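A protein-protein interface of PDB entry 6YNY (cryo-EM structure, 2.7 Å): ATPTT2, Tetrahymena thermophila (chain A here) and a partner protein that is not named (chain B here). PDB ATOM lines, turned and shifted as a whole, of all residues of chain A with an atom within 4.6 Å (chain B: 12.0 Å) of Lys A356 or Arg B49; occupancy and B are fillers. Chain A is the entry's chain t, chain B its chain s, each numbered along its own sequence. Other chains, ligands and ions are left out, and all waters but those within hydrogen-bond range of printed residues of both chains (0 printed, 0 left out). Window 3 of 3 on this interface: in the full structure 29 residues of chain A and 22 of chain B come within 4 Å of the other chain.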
ATOM      1  N   HIS A 349      16.811 -12.420  23.414  1.00  0.00           N
ATOM      2  CA  HIS A 349      17.428 -11.290  22.734  1.00  0.00           C
ATOM      3  C   HIS A 349      17.792 -11.637  21.301  1.00  0.00           C
ATOM      4  O   HIS A 349      17.737 -10.775  20.418  1.00  0.00           O
ATOM      5  CB  HIS A 349      18.677 -10.848  23.492  1.00  0.00           C
ATOM      6  CG  HIS A 349      18.414 -10.393  24.891  1.00  0.00           C
ATOM      7  ND1 HIS A 349      18.279  -9.064  25.227  1.00  0.00           N
ATOM      8  CD2 HIS A 349      18.271 -11.088  26.044  1.00  0.00           C
ATOM      9  CE1 HIS A 349      18.059  -8.960  26.524  1.00  0.00           C
ATOM     10  NE2 HIS A 349      18.049 -10.173  27.043  1.00  0.00           N
ATOM     11  N   ARG A 354      12.765  -6.374  20.188  1.00  0.00           N
ATOM     12  CA  ARG A 354      12.364  -5.335  21.123  1.00  0.00           C
ATOM     13  C   ARG A 354      12.547  -5.726  22.580  1.00  0.00           C
ATOM     14  O   ARG A 354      12.280  -4.903  23.461  1.00  0.00           O
ATOM     15  CB  ARG A 354      10.903  -4.951  20.883  1.00  0.00           C
ATOM     16  CG  ARG A 354      10.605  -4.482  19.478  1.00  0.00           C
ATOM     17  CD  ARG A 354      11.512  -3.345  19.057  1.00  0.00           C
ATOM     18  NE  ARG A 354      11.572  -2.280  20.049  1.00  0.00           N
ATOM     19  CZ  ARG A 354      12.389  -1.238  19.971  1.00  0.00           C
ATOM     20  NH1 ARG A 354      13.216  -1.118  18.949  1.00  0.00           N
ATOM     21  NH2 ARG A 354      12.380  -0.313  20.914  1.00  0.00           N
ATOM     22  N   VAL A 355      12.989  -6.947  22.861  1.00  0.00           N
ATOM     23  CA  VAL A 355      13.170  -7.375  24.244  1.00  0.00           C
ATOM     24  C   VAL A 355      14.272  -6.543  24.881  1.00  0.00           C
ATOM     25  O   VAL A 355      15.420  -6.544  24.421  1.00  0.00           O
ATOM     26  CB  VAL A 355      13.481  -8.872  24.314  1.00  0.00           C
ATOM     27  CG1 VAL A 355      14.045  -9.238  25.665  1.00  0.00           C
ATOM     28  CG2 VAL A 355      12.230  -9.660  24.051  1.00  0.00           C
ATOM     29  N   LYS A 356      13.922  -5.828  25.949  1.00  0.00           N
ATOM     30  CA  LYS A 356      14.878  -4.967  26.632  1.00  0.00           C
ATOM     31  C   LYS A 356      15.821  -5.776  27.510  1.00  0.00           C
ATOM     32  O   LYS A 356      17.039  -5.574  27.476  1.00  0.00           O
ATOM     33  CB  LYS A 356      14.132  -3.925  27.461  1.00  0.00           C
ATOM     34  CG  LYS A 356      15.025  -2.894  28.103  1.00  0.00           C
ATOM     35  CD  LYS A 356      14.234  -1.675  28.532  1.00  0.00           C
ATOM     36  CE  LYS A 356      15.039  -0.790  29.455  1.00  0.00           C
ATOM     37  NZ  LYS A 356      16.408  -0.569  28.946  1.00  0.00           N
ATOM     38  N   GLY A 357      15.281  -6.690  28.295  1.00  0.00           N
ATOM     39  CA  GLY A 357      16.098  -7.569  29.098  1.00  0.00           C
ATOM     40  C   GLY A 357      15.414  -7.918  30.402  1.00  0.00           C
ATOM     41  O   GLY A 357      14.238  -7.636  30.609  1.00  0.00           O
ATOM     42  N   HIS A 360      12.452  -6.067  32.751  1.00  0.00           N
ATOM     43  CA  HIS A 360      11.542  -5.263  31.950  1.00  0.00           C
ATOM     44  C   HIS A 360      10.611  -6.116  31.105  1.00  0.00           C
ATOM     45  O   HIS A 360       9.392  -5.930  31.141  1.00  0.00           O
ATOM     46  CB  HIS A 360      12.337  -4.319  31.041  1.00  0.00           C
ATOM     47  CG  HIS A 360      13.368  -3.512  31.761  1.00  0.00           C
ATOM     48  ND1 HIS A 360      14.686  -3.899  31.850  1.00  0.00           N
ATOM     49  CD2 HIS A 360      13.274  -2.338  32.428  1.00  0.00           C
ATOM     50  CE1 HIS A 360      15.361  -2.997  32.537  1.00  0.00           C
ATOM     51  NE2 HIS A 360      14.528  -2.040  32.901  1.00  0.00           N
ATOM     52  N   ASP A 361      11.163  -7.056  30.344  1.00  0.00           N
ATOM     53  CA  ASP A 361      10.382  -7.973  29.538  1.00  0.00           C
ATOM     54  C   ASP A 361      10.613  -9.429  29.905  1.00  0.00           C
ATOM     55  O   ASP A 361       9.907 -10.299  29.385  1.00  0.00           O
ATOM     56  CB  ASP A 361      10.703  -7.781  28.047  1.00  0.00           C
ATOM     57  CG  ASP A 361      10.537  -6.349  27.592  1.00  0.00           C
ATOM     58  OD1 ASP A 361      11.454  -5.538  27.835  1.00  0.00           O
ATOM     59  OD2 ASP A 361       9.492  -6.030  26.988  1.00  0.00           O
ATOM     60  N   LEU A 403       8.692   2.137  19.715  1.00  0.00           N
ATOM     61  CA  LEU A 403       9.460   3.243  20.263  1.00  0.00           C
ATOM     62  C   LEU A 403       8.740   3.957  21.396  1.00  0.00           C
ATOM     63  O   LEU A 403       9.326   4.847  22.018  1.00  0.00           O
ATOM     64  CB  LEU A 403       9.807   4.228  19.152  1.00  0.00           C
ATOM     65  CG  LEU A 403      10.658   3.636  18.033  1.00  0.00           C
ATOM     66  CD1 LEU A 403      10.803   4.615  16.897  1.00  0.00           C
ATOM     67  CD2 LEU A 403      12.019   3.233  18.555  1.00  0.00           C
ATOM     68  N   LYS A 405       7.184   3.852  25.185  1.00  0.00           N
ATOM     69  CA  LYS A 405       7.413   3.086  26.404  1.00  0.00           C
ATOM     70  C   LYS A 405       6.187   2.262  26.768  1.00  0.00           C
ATOM     71  O   LYS A 405       6.250   1.033  26.864  1.00  0.00           O
ATOM     72  CB  LYS A 405       7.771   4.024  27.554  1.00  0.00           C
ATOM     73  CG  LYS A 405       9.187   4.542  27.535  1.00  0.00           C
ATOM     74  CD  LYS A 405      10.222   3.449  27.714  1.00  0.00           C
ATOM     75  CE  LYS A 405      10.044   2.708  29.007  1.00  0.00           C
ATOM     76  NZ  LYS A 405      11.165   1.770  29.232  1.00  0.00           N
ATOM     77  N   GLU A 409       1.936   6.719  26.772  1.00  0.00           N
ATOM     78  CA  GLU A 409       2.546   7.638  25.822  1.00  0.00           C
ATOM     79  C   GLU A 409       1.746   7.792  24.539  1.00  0.00           C
ATOM     80  O   GLU A 409       2.132   8.595  23.683  1.00  0.00           O
ATOM     81  CB  GLU A 409       3.966   7.180  25.481  1.00  0.00           C
ATOM     82  CG  GLU A 409       4.983   7.479  26.558  1.00  0.00           C
ATOM     83  CD  GLU A 409       6.407   7.343  26.070  1.00  0.00           C
ATOM     84  OE1 GLU A 409       6.621   6.701  25.021  1.00  0.00           O
ATOM     85  OE2 GLU A 409       7.316   7.888  26.730  1.00  0.00           O
ATOM     86  N   PHE A 413       3.546  11.249  23.045  1.00  0.00           N
ATOM     87  CA  PHE A 413       4.931  11.057  22.651  1.00  0.00           C
ATOM     88  C   PHE A 413       5.009  10.978  21.136  1.00  0.00           C
ATOM     89  O   PHE A 413       4.277  10.204  20.512  1.00  0.00           O
ATOM     90  CB  PHE A 413       5.525   9.797  23.276  1.00  0.00           C
ATOM     91  CG  PHE A 413       6.988   9.629  23.008  1.00  0.00           C
ATOM     92  CD1 PHE A 413       7.921  10.264  23.796  1.00  0.00           C
ATOM     93  CD2 PHE A 413       7.430   8.844  21.964  1.00  0.00           C
ATOM     94  CE1 PHE A 413       9.263  10.118  23.550  1.00  0.00           C
ATOM     95  CE2 PHE A 413       8.773   8.695  21.714  1.00  0.00           C
ATOM     96  CZ  PHE A 413       9.689   9.332  22.509  1.00  0.00           C
ATOM     97  N   VAL B  44      12.614  -3.230  11.613  1.00  0.00           N
ATOM     98  CA  VAL B  44      12.281  -2.749  12.950  1.00  0.00           C
ATOM     99  C   VAL B  44      13.272  -1.671  13.362  1.00  0.00           C
ATOM    100  O   VAL B  44      14.461  -1.767  13.033  1.00  0.00           O
ATOM    101  CB  VAL B  44      12.292  -3.877  13.992  1.00  0.00           C
ATOM    102  CG1 VAL B  44      10.903  -4.312  14.293  1.00  0.00           C
ATOM    103  CG2 VAL B  44      13.141  -5.040  13.523  1.00  0.00           C
ATOM    104  N   PRO B  45      12.839  -0.640  14.078  1.00  0.00           N
ATOM    105  CA  PRO B  45      13.804   0.264  14.700  1.00  0.00           C
ATOM    106  C   PRO B  45      14.635  -0.471  15.739  1.00  0.00           C
ATOM    107  O   PRO B  45      14.122  -1.289  16.505  1.00  0.00           O
ATOM    108  CB  PRO B  45      12.922   1.342  15.334  1.00  0.00           C
ATOM    109  CG  PRO B  45      11.638   1.256  14.615  1.00  0.00           C
ATOM    110  CD  PRO B  45      11.458  -0.169  14.260  1.00  0.00           C
ATOM    111  N   TYR B  46      15.932  -0.176  15.754  1.00  0.00           N
ATOM    112  CA  TYR B  46      16.835  -0.842  16.678  1.00  0.00           C
ATOM    113  C   TYR B  46      16.807  -0.226  18.067  1.00  0.00           C
ATOM    114  O   TYR B  46      17.154  -0.906  19.038  1.00  0.00           O
ATOM    115  CB  TYR B  46      18.266  -0.797  16.140  1.00  0.00           C
ATOM    116  CG  TYR B  46      18.999   0.485  16.451  1.00  0.00           C
ATOM    117  CD1 TYR B  46      19.817   0.584  17.562  1.00  0.00           C
ATOM    118  CD2 TYR B  46      18.874   1.592  15.634  1.00  0.00           C
ATOM    119  CE1 TYR B  46      20.482   1.746  17.852  1.00  0.00           C
ATOM    120  CE2 TYR B  46      19.537   2.757  15.916  1.00  0.00           C
ATOM    121  CZ  TYR B  46      20.342   2.831  17.026  1.00  0.00           C
ATOM    122  OH  TYR B  46      21.015   3.993  17.320  1.00  0.00           O
ATOM    123  N   TYR B  47      16.395   1.030  18.180  1.00  0.00           N
ATOM    124  CA  TYR B  47      16.580   1.769  19.418  1.00  0.00           C
ATOM    125  C   TYR B  47      15.701   1.213  20.525  1.00  0.00           C
ATOM    126  O   TYR B  47      14.505   0.979  20.332  1.00  0.00           O
ATOM    127  CB  TYR B  47      16.278   3.245  19.200  1.00  0.00           C
ATOM    128  CG  TYR B  47      16.727   4.112  20.342  1.00  0.00           C
ATOM    129  CD1 TYR B  47      18.057   4.451  20.490  1.00  0.00           C
ATOM    130  CD2 TYR B  47      15.824   4.586  21.274  1.00  0.00           C
ATOM    131  CE1 TYR B  47      18.475   5.235  21.530  1.00  0.00           C
ATOM    132  CE2 TYR B  47      16.235   5.373  22.320  1.00  0.00           C
ATOM    133  CZ  TYR B  47      17.564   5.693  22.442  1.00  0.00           C
ATOM    134  OH  TYR B  47      17.994   6.479  23.478  1.00  0.00           O
ATOM    135  N   GLN B  48      16.304   1.010  21.689  1.00  0.00           N
ATOM    136  CA  GLN B  48      15.603   0.545  22.873  1.00  0.00           C
ATOM    137  C   GLN B  48      15.408   1.726  23.812  1.00  0.00           C
ATOM    138  O   GLN B  48      16.381   2.355  24.236  1.00  0.00           O
ATOM    139  CB  GLN B  48      16.383  -0.572  23.561  1.00  0.00           C
ATOM    140  CG  GLN B  48      15.692  -1.161  24.775  1.00  0.00           C
ATOM    141  CD  GLN B  48      14.326  -1.726  24.450  1.00  0.00           C
ATOM    142  OE1 GLN B  48      13.315  -1.309  25.016  1.00  0.00           O
ATOM    143  NE2 GLN B  48      14.288  -2.684  23.536  1.00  0.00           N
ATOM    144  N   ARG B  49      14.154   2.028  24.121  1.00  0.00           N
ATOM    145  CA  ARG B  49      13.855   3.149  24.996  1.00  0.00           C
ATOM    146  C   ARG B  49      14.421   2.897  26.386  1.00  0.00           C
ATOM    147  O   ARG B  49      14.214   1.834  26.976  1.00  0.00           O
ATOM    148  CB  ARG B  49      12.347   3.377  25.059  1.00  0.00           C
ATOM    149  CG  ARG B  49      11.783   4.048  23.828  1.00  0.00           C
ATOM    150  CD  ARG B  49      11.863   5.546  23.957  1.00  0.00           C
ATOM    151  NE  ARG B  49      10.728   6.077  24.698  1.00  0.00           N
ATOM    152  CZ  ARG B  49      10.707   7.271  25.275  1.00  0.00           C
ATOM    153  NH1 ARG B  49      11.760   8.071  25.206  1.00  0.00           N
ATOM    154  NH2 ARG B  49       9.623   7.660  25.928  1.00  0.00           N
ATOM    155  N   LEU B  50      15.149   3.884  26.901  1.00  0.00           N
ATOM    156  CA  LEU B  50      15.803   3.797  28.199  1.00  0.00           C
ATOM    157  C   LEU B  50      14.898   4.289  29.321  1.00  0.00           C
ATOM    158  O   LEU B  50      14.796   3.645  30.369  1.00  0.00           O
ATOM    159  CB  LEU B  50      17.096   4.611  28.177  1.00  0.00           C
ATOM    160  CG  LEU B  50      18.098   4.244  27.088  1.00  0.00           C
ATOM    161  CD1 LEU B  50      19.151   5.319  26.957  1.00  0.00           C
ATOM    162  CD2 LEU B  50      18.736   2.905  27.382  1.00  0.00           C
ATOM    163  N   PHE B  51      14.248   5.429  29.116  1.00  0.00           N
ATOM    164  CA  PHE B  51      13.419   6.053  30.131  1.00  0.00           C
ATOM    165  C   PHE B  51      12.125   6.536  29.502  1.00  0.00           C
ATOM    166  O   PHE B  51      12.009   6.659  28.281  1.00  0.00           O
ATOM    167  CB  PHE B  51      14.126   7.238  30.797  1.00  0.00           C
ATOM    168  CG  PHE B  51      15.366   6.867  31.539  1.00  0.00           C
ATOM    169  CD1 PHE B  51      15.293   6.261  32.776  1.00  0.00           C
ATOM    170  CD2 PHE B  51      16.607   7.138  31.007  1.00  0.00           C
ATOM    171  CE1 PHE B  51      16.432   5.924  33.459  1.00  0.00           C
ATOM    172  CE2 PHE B  51      17.748   6.802  31.685  1.00  0.00           C
ATOM    173  CZ  PHE B  51      17.662   6.196  32.914  1.00  0.00           C
ATOM    174  N   LYS B  52      11.149   6.812  30.358  1.00  0.00           N
ATOM    175  CA  LYS B  52       9.919   7.439  29.915  1.00  0.00           C
ATOM    176  C   LYS B  52      10.114   8.942  29.821  1.00  0.00           C
ATOM    177  O   LYS B  52      10.744   9.559  30.682  1.00  0.00           O
ATOM    178  CB  LYS B  52       8.772   7.122  30.870  1.00  0.00           C
ATOM    179  CG  LYS B  52       7.472   7.797  30.497  1.00  0.00           C
ATOM    180  CD  LYS B  52       6.406   7.559  31.527  1.00  0.00           C
ATOM    181  CE  LYS B  52       5.221   8.470  31.298  1.00  0.00           C
ATOM    182  NZ  LYS B  52       4.763   8.407  29.890  1.00  0.00           N
ATOM    183  N   ALA B  53       9.563   9.528  28.767  1.00  0.00           N
ATOM    184  CA  ALA B  53       9.661  10.964  28.573  1.00  0.00           C
ATOM    185  C   ALA B  53       8.885  11.701  29.653  1.00  0.00           C
ATOM    186  O   ALA B  53       7.747  11.346  29.972  1.00  0.00           O
ATOM    187  CB  ALA B  53       9.136  11.341  27.194  1.00  0.00           C
ATOM    188  N   TYR B  54       9.510  12.731  30.217  1.00  0.00           N
ATOM    189  CA  TYR B  54       8.896  13.559  31.254  1.00  0.00           C
ATOM    190  C   TYR B  54       9.265  15.010  30.982  1.00  0.00           C
ATOM    191  O   TYR B  54       9.970  15.653  31.762  1.00  0.00           O
ATOM    192  CB  TYR B  54       9.345  13.109  32.642  1.00  0.00           C
ATOM    193  CG  TYR B  54       8.486  13.622  33.773  1.00  0.00           C
ATOM    194  CD1 TYR B  54       7.110  13.488  33.740  1.00  0.00           C
ATOM    195  CD2 TYR B  54       9.056  14.212  34.888  1.00  0.00           C
ATOM    196  CE1 TYR B  54       6.327  13.944  34.768  1.00  0.00           C
ATOM    197  CE2 TYR B  54       8.277  14.669  35.923  1.00  0.00           C
ATOM    198  CZ  TYR B  54       6.914  14.530  35.859  1.00  0.00           C
ATOM    199  OH  TYR B  54       6.135  14.988  36.891  1.00  0.00           O
ATOM    200  N   PRO B  55       8.797  15.557  29.859  1.00  0.00           N
ATOM    201  CA  PRO B  55       9.210  16.917  29.490  1.00  0.00           C
ATOM    202  C   PRO B  55       8.648  17.984  30.403  1.00  0.00           C
ATOM    203  O   PRO B  55       9.336  18.970  30.696  1.00  0.00           O
ATOM    204  CB  PRO B  55       8.678  17.057  28.060  1.00  0.00           C
ATOM    205  CG  PRO B  55       7.524  16.131  28.001  1.00  0.00           C
ATOM    206  CD  PRO B  55       7.862  14.976  28.884  1.00  0.00           C
ATOM    207  N   ILE B  56       7.412  17.822  30.858  1.00  0.00           N
ATOM    208  CA  ILE B  56       6.746  18.793  31.712  1.00  0.00           C
ATOM    209  C   ILE B  56       6.460  18.129  33.047  1.00  0.00           C
ATOM    210  O   ILE B  56       5.894  17.031  33.093  1.00  0.00           O
ATOM    211  CB  ILE B  56       5.453  19.321  31.068  1.00  0.00           C
ATOM    212  CG1 ILE B  56       5.717  19.720  29.620  1.00  0.00           C
ATOM    213  CG2 ILE B  56       4.939  20.511  31.830  1.00  0.00           C
ATOM    214  CD1 ILE B  56       4.528  20.284  28.924  1.00  0.00           C
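The guanidinium group (NH2) of Arg A354 sits at hydrogen-bond distance from the backbone carbonyl oxygen (O) of Tyr B47 (2.6 Å). NH2 of Arg B49 lies within salt-bridge range of OE2 of Glu A409 (2.5 Å). The backbone NH (N) of Ala B53 is in hydrogen-bond range of the side-chain carboxylate (OE2) of Glu A409, 3.4 Å away. O of Leu A403 sits close to NE of Arg B49, at 3.3 Å. The backbone carbonyl oxygen (O) of Arg A354 lies within hydrogen-bond range of the side-chain amide nitrogen (NE2) of Gln B48 (3.0 Å). NH1 of Arg A354 sits at hydrogen-bond distance from O of Pro B45.
N of Lys A405 lies within hydrogen-bond range of OE1 of Glu A409 (2.9 Å). NH1 of Arg B49 lies close to O of Phe B51, 3.4 Å away. N of Lys A356 sits at hydrogen-bond distance from OD1 of Asp A361.
NH1 of Arg A354 touches C of Tyr B46, at 3.8 Å. Gln B48 touches Lys A356. Leu A403 touches Pro B45 (CD2 to CB, 3.8 Å). Tyr B47 touches Leu A403 (O to CD2, 3.8 Å). Lys A405 touches Arg B49. CG of Lys A405 touches O of Phe B51, 3.6 Å away. Lys B52 touches Lys A405. NZ of Lys B52 touches CG of Glu A409, 3.5 Å away. NH2 of Arg B49 touches CE1 of Phe A413, 3.4 Å away. Ala B53 touches Phe A413 (CB to CD1, 3.8 Å).
No residue of chain B comes within 4 Å of Val A355. Lys A356 touches just these residues of chain B: Gln B48 (3.7 Å) and Arg B49 (3.7 Å). No residue of chain B comes within 4 Å of Asp A361. Of chain B, only Pro B45, Tyr B47 and Arg B49 come within 4 Å of Leu A403. Printed residues of chain B within 4 Å of Glu A409: Arg B49, Lys B52 and Ala B53. Of the printed residues of chain A, Pro B45 touches Arg A354 and Leu A403. Of the printed residues of chain A, Tyr B47 touches Arg A354 (2.6 Å) and Leu A403 (3.8 Å). Arg B49 touches five residues of chain A. Of the printed residues of chain A, Lys B52 touches Lys A405 (3.8 Å) and Glu A409 (3.5 Å). Tyr B54 touches none of the printed residues of chain A. The nearest residue of chain B that does not touch Lys A356 is Leu B50 (4.5 Å). The nearest printed residue of chain A that does not touch Phe B51 is Glu A409 (5.1 Å).
Printed residues of chain A that touch a printed residue of chain B: Arg A354, Lys A356, Leu A403, Lys A405, Glu A409 and Phe A413. Hydrophobic or aromatic side chains of chain A that line the printed part of chain B: Leu A403 and Phe A413. Among the printed residues, 17 pairs touch across the chains. Among the printed residues, Asp or Glu carboxylates within 4 Å of a Lys or Arg side-chain nitrogen of the other chain: Glu A409 with Arg B49 (2.5 Å).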
